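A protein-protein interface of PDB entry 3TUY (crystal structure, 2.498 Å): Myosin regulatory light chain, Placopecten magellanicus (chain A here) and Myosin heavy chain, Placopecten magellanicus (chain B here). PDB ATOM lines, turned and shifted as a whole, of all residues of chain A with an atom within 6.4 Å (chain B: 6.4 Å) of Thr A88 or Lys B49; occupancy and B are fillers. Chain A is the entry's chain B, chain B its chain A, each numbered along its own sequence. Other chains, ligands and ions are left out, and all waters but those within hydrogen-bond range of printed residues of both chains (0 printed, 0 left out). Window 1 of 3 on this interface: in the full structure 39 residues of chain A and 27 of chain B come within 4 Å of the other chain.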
ATOM      1  N   ARG A  16      -9.953 -26.179 -11.201  1.00  0.00           N
ATOM      2  CA  ARG A  16     -10.756 -25.579 -12.265  1.00  0.00           C
ATOM      3  C   ARG A  16     -11.834 -24.632 -11.703  1.00  0.00           C
ATOM      4  O   ARG A  16     -12.444 -24.936 -10.675  1.00  0.00           O
ATOM      5  CB  ARG A  16     -11.412 -26.669 -13.115  1.00  0.00           C
ATOM      6  CG  ARG A  16     -10.428 -27.501 -13.923  1.00  0.00           C
ATOM      7  CD  ARG A  16     -11.083 -28.553 -14.804  1.00  0.00           C
ATOM      8  NE  ARG A  16     -10.097 -29.371 -15.505  1.00  0.00           N
ATOM      9  CZ  ARG A  16     -10.397 -30.428 -16.245  1.00  0.00           C
ATOM     10  NH1 ARG A  16     -11.662 -30.803 -16.390  1.00  0.00           N
ATOM     11  NH2 ARG A  16      -9.433 -31.114 -16.847  1.00  0.00           N
ATOM     12  N   PRO A  18      -9.176 -21.828 -13.560  1.00  0.00           N
ATOM     13  CA  PRO A  18      -8.132 -20.917 -13.057  1.00  0.00           C
ATOM     14  C   PRO A  18      -8.440 -19.426 -13.172  1.00  0.00           C
ATOM     15  O   PRO A  18      -9.162 -19.008 -14.068  1.00  0.00           O
ATOM     16  CB  PRO A  18      -6.906 -21.276 -13.907  1.00  0.00           C
ATOM     17  CG  PRO A  18      -7.432 -22.032 -15.065  1.00  0.00           C
ATOM     18  CD  PRO A  18      -8.656 -22.739 -14.590  1.00  0.00           C
ATOM     19  N   LEU A  21      -7.674 -17.362 -16.355  1.00  0.00           N
ATOM     20  CA  LEU A  21      -8.648 -17.675 -17.390  1.00  0.00           C
ATOM     21  C   LEU A  21      -9.954 -16.915 -17.156  1.00  0.00           C
ATOM     22  O   LEU A  21     -10.590 -16.445 -18.106  1.00  0.00           O
ATOM     23  CB  LEU A  21      -8.917 -19.179 -17.409  1.00  0.00           C
ATOM     24  CG  LEU A  21      -9.813 -19.733 -18.515  1.00  0.00           C
ATOM     25  CD1 LEU A  21      -9.274 -19.364 -19.885  1.00  0.00           C
ATOM     26  CD2 LEU A  21      -9.923 -21.243 -18.381  1.00  0.00           C
ATOM     27  N   GLU A  24      -9.321 -13.445 -18.187  1.00  0.00           N
ATOM     28  CA  GLU A  24      -9.357 -13.356 -19.632  1.00  0.00           C
ATOM     29  C   GLU A  24     -10.804 -13.328 -20.149  1.00  0.00           C
ATOM     30  O   GLU A  24     -11.152 -12.521 -21.015  1.00  0.00           O
ATOM     31  CB  GLU A  24      -8.589 -14.520 -20.235  1.00  0.00           C
ATOM     32  CG  GLU A  24      -8.685 -14.609 -21.739  1.00  0.00           C
ATOM     33  CD  GLU A  24      -7.893 -15.774 -22.283  1.00  0.00           C
ATOM     34  OE1 GLU A  24      -6.653 -15.624 -22.437  1.00  0.00           O
ATOM     35  OE2 GLU A  24      -8.512 -16.839 -22.543  1.00  0.00           O
ATOM     36  N   ASP A  83     -17.437 -24.346 -19.731  1.00  0.00           N
ATOM     37  CA  ASP A  83     -17.194 -25.757 -19.935  1.00  0.00           C
ATOM     38  C   ASP A  83     -16.284 -25.939 -21.126  1.00  0.00           C
ATOM     39  O   ASP A  83     -15.376 -26.766 -21.104  1.00  0.00           O
ATOM     40  CB  ASP A  83     -18.509 -26.527 -20.131  1.00  0.00           C
ATOM     41  CG  ASP A  83     -19.399 -26.478 -18.904  1.00  0.00           C
ATOM     42  OD1 ASP A  83     -18.897 -26.715 -17.781  1.00  0.00           O
ATOM     43  OD2 ASP A  83     -20.602 -26.176 -19.055  1.00  0.00           O
ATOM     44  N   LYS A  84     -16.509 -25.151 -22.165  1.00  0.00           N
ATOM     45  CA  LYS A  84     -15.711 -25.294 -23.377  1.00  0.00           C
ATOM     46  C   LYS A  84     -14.246 -24.851 -23.197  1.00  0.00           C
ATOM     47  O   LYS A  84     -13.364 -25.356 -23.868  1.00  0.00           O
ATOM     48  CB  LYS A  84     -16.391 -24.619 -24.583  1.00  0.00           C
ATOM     49  CG  LYS A  84     -17.704 -25.309 -24.955  1.00  0.00           C
ATOM     50  CD  LYS A  84     -18.209 -24.972 -26.362  1.00  0.00           C
ATOM     51  CE  LYS A  84     -19.636 -25.505 -26.610  1.00  0.00           C
ATOM     52  NZ  LYS A  84     -20.657 -24.727 -25.841  1.00  0.00           N
ATOM     53  N   LEU A  85     -13.993 -23.942 -22.267  1.00  0.00           N
ATOM     54  CA  LEU A  85     -12.643 -23.437 -22.041  1.00  0.00           C
ATOM     55  C   LEU A  85     -11.938 -24.040 -20.836  1.00  0.00           C
ATOM     56  O   LEU A  85     -10.738 -23.876 -20.691  1.00  0.00           O
ATOM     57  CB  LEU A  85     -12.663 -21.922 -21.866  1.00  0.00           C
ATOM     58  CG  LEU A  85     -13.104 -21.108 -23.082  1.00  0.00           C
ATOM     59  CD1 LEU A  85     -12.684 -19.693 -22.898  1.00  0.00           C
ATOM     60  CD2 LEU A  85     -12.516 -21.671 -24.368  1.00  0.00           C
ATOM     61  N   SER A  86     -12.672 -24.752 -19.987  1.00  0.00           N
ATOM     62  CA  SER A  86     -12.171 -25.057 -18.653  1.00  0.00           C
ATOM     63  C   SER A  86     -10.833 -25.794 -18.642  1.00  0.00           C
ATOM     64  O   SER A  86      -9.986 -25.556 -17.759  1.00  0.00           O
ATOM     65  CB  SER A  86     -13.210 -25.819 -17.834  1.00  0.00           C
ATOM     66  OG  SER A  86     -13.442 -27.086 -18.416  1.00  0.00           O
ATOM     67  N   GLY A  87     -10.626 -26.682 -19.607  1.00  0.00           N
ATOM     68  CA  GLY A  87      -9.367 -27.415 -19.632  1.00  0.00           C
ATOM     69  C   GLY A  87      -8.319 -26.896 -20.606  1.00  0.00           C
ATOM     70  O   GLY A  87      -7.407 -27.627 -20.967  1.00  0.00           O
ATOM     71  N   THR A  88      -8.428 -25.648 -21.049  1.00  0.00           N
ATOM     72  CA  THR A  88      -7.514 -25.184 -22.089  1.00  0.00           C
ATOM     73  C   THR A  88      -6.320 -24.486 -21.481  1.00  0.00           C
ATOM     74  O   THR A  88      -6.390 -24.014 -20.348  1.00  0.00           O
ATOM     75  CB  THR A  88      -8.200 -24.301 -23.147  1.00  0.00           C
ATOM     76  OG1 THR A  88      -8.620 -23.055 -22.571  1.00  0.00           O
ATOM     77  CG2 THR A  88      -9.398 -25.036 -23.730  1.00  0.00           C
ATOM     78  N   ASP A  89      -5.219 -24.457 -22.225  1.00  0.00           N
ATOM     79  CA  ASP A  89      -3.971 -23.899 -21.723  1.00  0.00           C
ATOM     80  C   ASP A  89      -3.425 -22.907 -22.708  1.00  0.00           C
ATOM     81  O   ASP A  89      -3.792 -22.912 -23.885  1.00  0.00           O
ATOM     82  CB  ASP A  89      -2.931 -24.990 -21.482  1.00  0.00           C
ATOM     83  CG  ASP A  89      -3.419 -26.065 -20.514  1.00  0.00           C
ATOM     84  OD1 ASP A  89      -3.400 -25.804 -19.289  1.00  0.00           O
ATOM     85  OD2 ASP A  89      -3.813 -27.171 -20.967  1.00  0.00           O
ATOM     86  N   SER A  90      -2.537 -22.052 -22.219  1.00  0.00           N
ATOM     87  CA  SER A  90      -1.937 -21.029 -23.059  1.00  0.00           C
ATOM     88  C   SER A  90      -1.056 -21.684 -24.110  1.00  0.00           C
ATOM     89  O   SER A  90      -0.533 -22.788 -23.914  1.00  0.00           O
ATOM     90  CB  SER A  90      -1.087 -20.075 -22.217  1.00  0.00           C
ATOM     91  OG  SER A  90       0.116 -20.707 -21.829  1.00  0.00           O
ATOM     92  N   ILE A  94       1.255 -25.228 -23.954  1.00  0.00           N
ATOM     93  CA  ILE A  94       1.121 -26.307 -24.910  1.00  0.00           C
ATOM     94  C   ILE A  94       2.427 -26.559 -25.678  1.00  0.00           C
ATOM     95  O   ILE A  94       2.771 -27.707 -25.945  1.00  0.00           O
ATOM     96  CB  ILE A  94      -0.088 -26.085 -25.850  1.00  0.00           C
ATOM     97  CG1 ILE A  94      -1.353 -25.865 -25.024  1.00  0.00           C
ATOM     98  CG2 ILE A  94      -0.309 -27.279 -26.760  1.00  0.00           C
ATOM     99  CD1 ILE A  94      -2.586 -25.639 -25.842  1.00  0.00           C
ATOM    100  N   LYS A 154      -5.067 -22.471 -31.550  1.00  0.00           N
ATOM    101  CA  LYS A 154      -5.401 -21.361 -30.675  1.00  0.00           C
ATOM    102  C   LYS A 154      -6.089 -20.218 -31.411  1.00  0.00           C
ATOM    103  O   LYS A 154      -6.607 -19.312 -30.764  1.00  0.00           O
ATOM    104  CB  LYS A 154      -4.163 -20.821 -29.955  1.00  0.00           C
ATOM    105  CG  LYS A 154      -3.424 -21.823 -29.061  1.00  0.00           C
ATOM    106  CD  LYS A 154      -4.297 -22.382 -27.947  1.00  0.00           C
ATOM    107  CE  LYS A 154      -4.464 -21.396 -26.816  1.00  0.00           C
ATOM    108  NZ  LYS A 154      -5.345 -21.997 -25.779  1.00  0.00           N
ATOM    109  N   GLN B  44      -3.377 -33.734 -25.409  1.00  0.00           N
ATOM    110  CA  GLN B  44      -4.594 -34.445 -25.855  1.00  0.00           C
ATOM    111  C   GLN B  44      -5.852 -33.646 -25.516  1.00  0.00           C
ATOM    112  O   GLN B  44      -6.804 -33.589 -26.297  1.00  0.00           O
ATOM    113  CB  GLN B  44      -4.680 -35.893 -25.303  1.00  0.00           C
ATOM    114  CG  GLN B  44      -3.553 -36.834 -25.810  1.00  0.00           C
ATOM    115  CD  GLN B  44      -3.494 -38.227 -25.130  1.00  0.00           C
ATOM    116  OE1 GLN B  44      -3.568 -38.374 -23.899  1.00  0.00           O
ATOM    117  NE2 GLN B  44      -3.355 -39.255 -25.954  1.00  0.00           N
ATOM    118  N   ARG B  45      -5.837 -33.013 -24.350  1.00  0.00           N
ATOM    119  CA  ARG B  45      -6.978 -32.247 -23.886  1.00  0.00           C
ATOM    120  C   ARG B  45      -7.218 -31.020 -24.746  1.00  0.00           C
ATOM    121  O   ARG B  45      -8.344 -30.738 -25.138  1.00  0.00           O
ATOM    122  CB  ARG B  45      -6.734 -31.812 -22.454  1.00  0.00           C
ATOM    123  CG  ARG B  45      -7.758 -30.872 -21.924  1.00  0.00           C
ATOM    124  CD  ARG B  45      -7.526 -30.665 -20.449  1.00  0.00           C
ATOM    125  NE  ARG B  45      -6.318 -29.888 -20.195  1.00  0.00           N
ATOM    126  CZ  ARG B  45      -5.343 -30.267 -19.379  1.00  0.00           C
ATOM    127  NH1 ARG B  45      -5.429 -31.429 -18.740  1.00  0.00           N
ATOM    128  NH2 ARG B  45      -4.284 -29.482 -19.205  1.00  0.00           N
ATOM    129  N   ASN B  46      -6.144 -30.293 -25.034  1.00  0.00           N
ATOM    130  CA  ASN B  46      -6.221 -29.097 -25.860  1.00  0.00           C
ATOM    131  C   ASN B  46      -6.577 -29.349 -27.320  1.00  0.00           C
ATOM    132  O   ASN B  46      -7.332 -28.584 -27.919  1.00  0.00           O
ATOM    133  CB  ASN B  46      -4.941 -28.263 -25.745  1.00  0.00           C
ATOM    134  CG  ASN B  46      -4.916 -27.443 -24.490  1.00  0.00           C
ATOM    135  OD1 ASN B  46      -5.558 -26.402 -24.399  1.00  0.00           O
ATOM    136  ND2 ASN B  46      -4.193 -27.916 -23.503  1.00  0.00           N
ATOM    137  N   ILE B  47      -6.041 -30.408 -27.906  1.00  0.00           N
ATOM    138  CA  ILE B  47      -6.462 -30.762 -29.243  1.00  0.00           C
ATOM    139  C   ILE B  47      -7.949 -31.098 -29.200  1.00  0.00           C
ATOM    140  O   ILE B  47      -8.713 -30.633 -30.035  1.00  0.00           O
ATOM    141  CB  ILE B  47      -5.660 -31.954 -29.815  1.00  0.00           C
ATOM    142  CG1 ILE B  47      -4.162 -31.608 -29.900  1.00  0.00           C
ATOM    143  CG2 ILE B  47      -6.243 -32.370 -31.165  1.00  0.00           C
ATOM    144  CD1 ILE B  47      -3.262 -32.775 -30.259  1.00  0.00           C
ATOM    145  N   ARG B  48      -8.365 -31.890 -28.215  1.00  0.00           N
ATOM    146  CA  ARG B  48      -9.776 -32.232 -28.109  1.00  0.00           C
ATOM    147  C   ARG B  48     -10.701 -31.002 -27.954  1.00  0.00           C
ATOM    148  O   ARG B  48     -11.789 -30.971 -28.521  1.00  0.00           O
ATOM    149  CB  ARG B  48     -10.022 -33.264 -27.002  1.00  0.00           C
ATOM    150  CG  ARG B  48      -9.875 -34.694 -27.479  1.00  0.00           C
ATOM    151  CD  ARG B  48      -9.798 -35.696 -26.319  1.00  0.00           C
ATOM    152  NE  ARG B  48      -9.872 -37.068 -26.819  1.00  0.00           N
ATOM    153  CZ  ARG B  48      -9.149 -38.087 -26.357  1.00  0.00           C
ATOM    154  NH1 ARG B  48      -8.281 -37.892 -25.357  1.00  0.00           N
ATOM    155  NH2 ARG B  48      -9.291 -39.302 -26.899  1.00  0.00           N
ATOM    156  N   LYS B  49     -10.264 -29.992 -27.204  1.00  0.00           N
ATOM    157  CA  LYS B  49     -11.051 -28.763 -27.046  1.00  0.00           C
ATOM    158  C   LYS B  49     -11.210 -28.074 -28.400  1.00  0.00           C
ATOM    159  O   LYS B  49     -12.326 -27.764 -28.833  1.00  0.00           O
ATOM    160  CB  LYS B  49     -10.389 -27.801 -26.051  1.00  0.00           C
ATOM    161  CG  LYS B  49     -10.403 -28.267 -24.598  1.00  0.00           C
ATOM    162  CD  LYS B  49     -11.814 -28.422 -24.091  1.00  0.00           C
ATOM    163  CE  LYS B  49     -11.836 -28.899 -22.655  1.00  0.00           C
ATOM    164  NZ  LYS B  49     -13.229 -29.180 -22.189  1.00  0.00           N
ATOM    165  N   TRP B  50     -10.078 -27.839 -29.059  1.00  0.00           N
ATOM    166  CA  TRP B  50     -10.070 -27.291 -30.403  1.00  0.00           C
ATOM    167  C   TRP B  50     -11.102 -27.965 -31.333  1.00  0.00           C
ATOM    168  O   TRP B  50     -11.946 -27.286 -31.911  1.00  0.00           O
ATOM    169  CB  TRP B  50      -8.661 -27.394 -30.977  1.00  0.00           C
ATOM    170  CG  TRP B  50      -8.540 -26.930 -32.375  1.00  0.00           C
ATOM    171  CD1 TRP B  50      -8.743 -25.665 -32.838  1.00  0.00           C
ATOM    172  CD2 TRP B  50      -8.154 -27.714 -33.503  1.00  0.00           C
ATOM    173  NE1 TRP B  50      -8.519 -25.612 -34.185  1.00  0.00           N
ATOM    174  CE2 TRP B  50      -8.155 -26.855 -34.624  1.00  0.00           C
ATOM    175  CE3 TRP B  50      -7.804 -29.062 -33.678  1.00  0.00           C
ATOM    176  CZ2 TRP B  50      -7.815 -27.296 -35.906  1.00  0.00           C
ATOM    177  CZ3 TRP B  50      -7.477 -29.502 -34.960  1.00  0.00           C
ATOM    178  CH2 TRP B  50      -7.480 -28.622 -36.053  1.00  0.00           C
ATOM    179  N   LEU B  51     -11.045 -29.294 -31.457  1.00  0.00           N
ATOM    180  CA  LEU B  51     -11.903 -30.045 -32.385  1.00  0.00           C
ATOM    181  C   LEU B  51     -13.388 -29.803 -32.170  1.00  0.00           C
ATOM    182  O   LEU B  51     -14.199 -29.912 -33.088  1.00  0.00           O
ATOM    183  CB  LEU B  51     -11.647 -31.541 -32.241  1.00  0.00           C
ATOM    184  CG  LEU B  51     -10.248 -32.063 -32.582  1.00  0.00           C
ATOM    185  CD1 LEU B  51     -10.195 -33.532 -32.334  1.00  0.00           C
ATOM    186  CD2 LEU B  51      -9.897 -31.748 -34.025  1.00  0.00           C
ATOM    187  N   VAL B  52     -13.742 -29.489 -30.940  1.00  0.00           N
ATOM    188  CA  VAL B  52     -15.127 -29.263 -30.604  1.00  0.00           C
ATOM    189  C   VAL B  52     -15.486 -27.812 -30.871  1.00  0.00           C
ATOM    190  O   VAL B  52     -16.545 -27.482 -31.422  1.00  0.00           O
ATOM    191  CB  VAL B  52     -15.379 -29.581 -29.110  1.00  0.00           C
ATOM    192  CG1 VAL B  52     -16.495 -28.711 -28.567  1.00  0.00           C
ATOM    193  CG2 VAL B  52     -15.698 -31.059 -28.937  1.00  0.00           C
ATOM    194  N   LEU B  53     -14.564 -26.948 -30.501  1.00  0.00           N
ATOM    195  CA  LEU B  53     -14.835 -25.539 -30.418  1.00  0.00           C
ATOM    196  C   LEU B  53     -14.494 -24.737 -31.705  1.00  0.00           C
ATOM    197  O   LEU B  53     -14.914 -23.589 -31.850  1.00  0.00           O
ATOM    198  CB  LEU B  53     -14.172 -25.017 -29.135  1.00  0.00           C
ATOM    199  CG  LEU B  53     -13.293 -23.789 -28.949  1.00  0.00           C
ATOM    200  CD1 LEU B  53     -12.764 -23.702 -27.488  1.00  0.00           C
ATOM    201  CD2 LEU B  53     -12.146 -23.829 -29.947  1.00  0.00           C
ATOM    202  N   ARG B  54     -13.808 -25.356 -32.662  1.00  0.00           N
ATOM    203  CA  ARG B  54     -13.298 -24.628 -33.820  1.00  0.00           C
ATOM    204  C   ARG B  54     -14.346 -24.201 -34.859  1.00  0.00           C
ATOM    205  O   ARG B  54     -14.069 -23.337 -35.670  1.00  0.00           O
ATOM    206  CB  ARG B  54     -12.229 -25.446 -34.528  1.00  0.00           C
ATOM    207  CG  ARG B  54     -12.815 -26.599 -35.321  1.00  0.00           C
ATOM    208  CD  ARG B  54     -11.743 -27.372 -36.076  1.00  0.00           C
ATOM    209  NE  ARG B  54     -12.272 -28.620 -36.609  1.00  0.00           N
ATOM    210  CZ  ARG B  54     -11.510 -29.618 -37.044  1.00  0.00           C
ATOM    211  NH1 ARG B  54     -10.194 -29.504 -37.007  1.00  0.00           N
ATOM    212  NH2 ARG B  54     -12.054 -30.733 -37.510  1.00  0.00           N
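The guanidinium group (NH2) of Arg B45 is in salt-bridge range of the side-chain carboxylate (OD2) of Asp A89, 2.9 Å away. NE of Arg B45 lies within hydrogen-bond range of O of Gly A87 (2.6 Å). The side-chain amide nitrogen (ND2) of Asn B46 lies within hydrogen-bond range of the side-chain carboxylate (OD2) of Asp A89 (2.7 Å). The side-chain amino group (NZ) of Lys B49 sits at hydrogen-bond distance from the backbone carbonyl oxygen (O) of Asp A83, 3.4 Å away.
O of Leu A85 lies within hydrogen-bond range of OG1 of Thr A88, 2.9 Å away. The backbone carbonyl oxygen (O) of Asp A89 is in hydrogen-bond range of the side-chain amino group (NZ) of Lys A154. The backbone carbonyl oxygen (O) of Asp A83 is in hydrogen-bond range of the side-chain hydroxyl (OG) of Ser A86, 3.3 Å away.
Among the printed residues, merely in contact across the chains: Ile A94 with Asn B46, Thr A88 with Asn B46, Lys A84 with Lys B49, Thr A88 with Lys B49, Leu A85 with Leu B53 and Gly A87 with Lys B49.
Of chain B, only Asn B46 (3.3 Å) and Lys B49 (3.5 Å) come within 4 Å of Thr A88. Of chain A, only Asp A83, Lys A84, Gly A87 and Thr A88 come within 4 Å of Lys B49. Of the printed residues of chain B, Asp A89 touches Arg B45 (2.9 Å) and Asn B46 (2.7 Å). Of the printed residues of chain B, Gly A87 touches Arg B45 (2.6 Å) and Lys B49 (3.96 Å). Arg A16 touches none of the printed residues of chain B. The nearest residue of chain B that does not touch Thr A88 is Arg B45 (4.8 Å). The nearest residue of chain A that does not touch Lys B49 is Ser A86 (4.3 Å). The nearest printed residue of chain B that does not touch Gly A87 is Asn B46 (4.1 Å).
Printed residues of chain B that touch a printed residue of chain A: Arg B45, Asn B46, Lys B49 and Leu B53. Along chain B the printed residues that touch a printed residue of chain A span positions 45 to 53. Of the 14 printed residues of chain A, 7 touch a printed residue of chain B. Along chain A the printed residues that touch a printed residue of chain B span positions 83 to 94.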
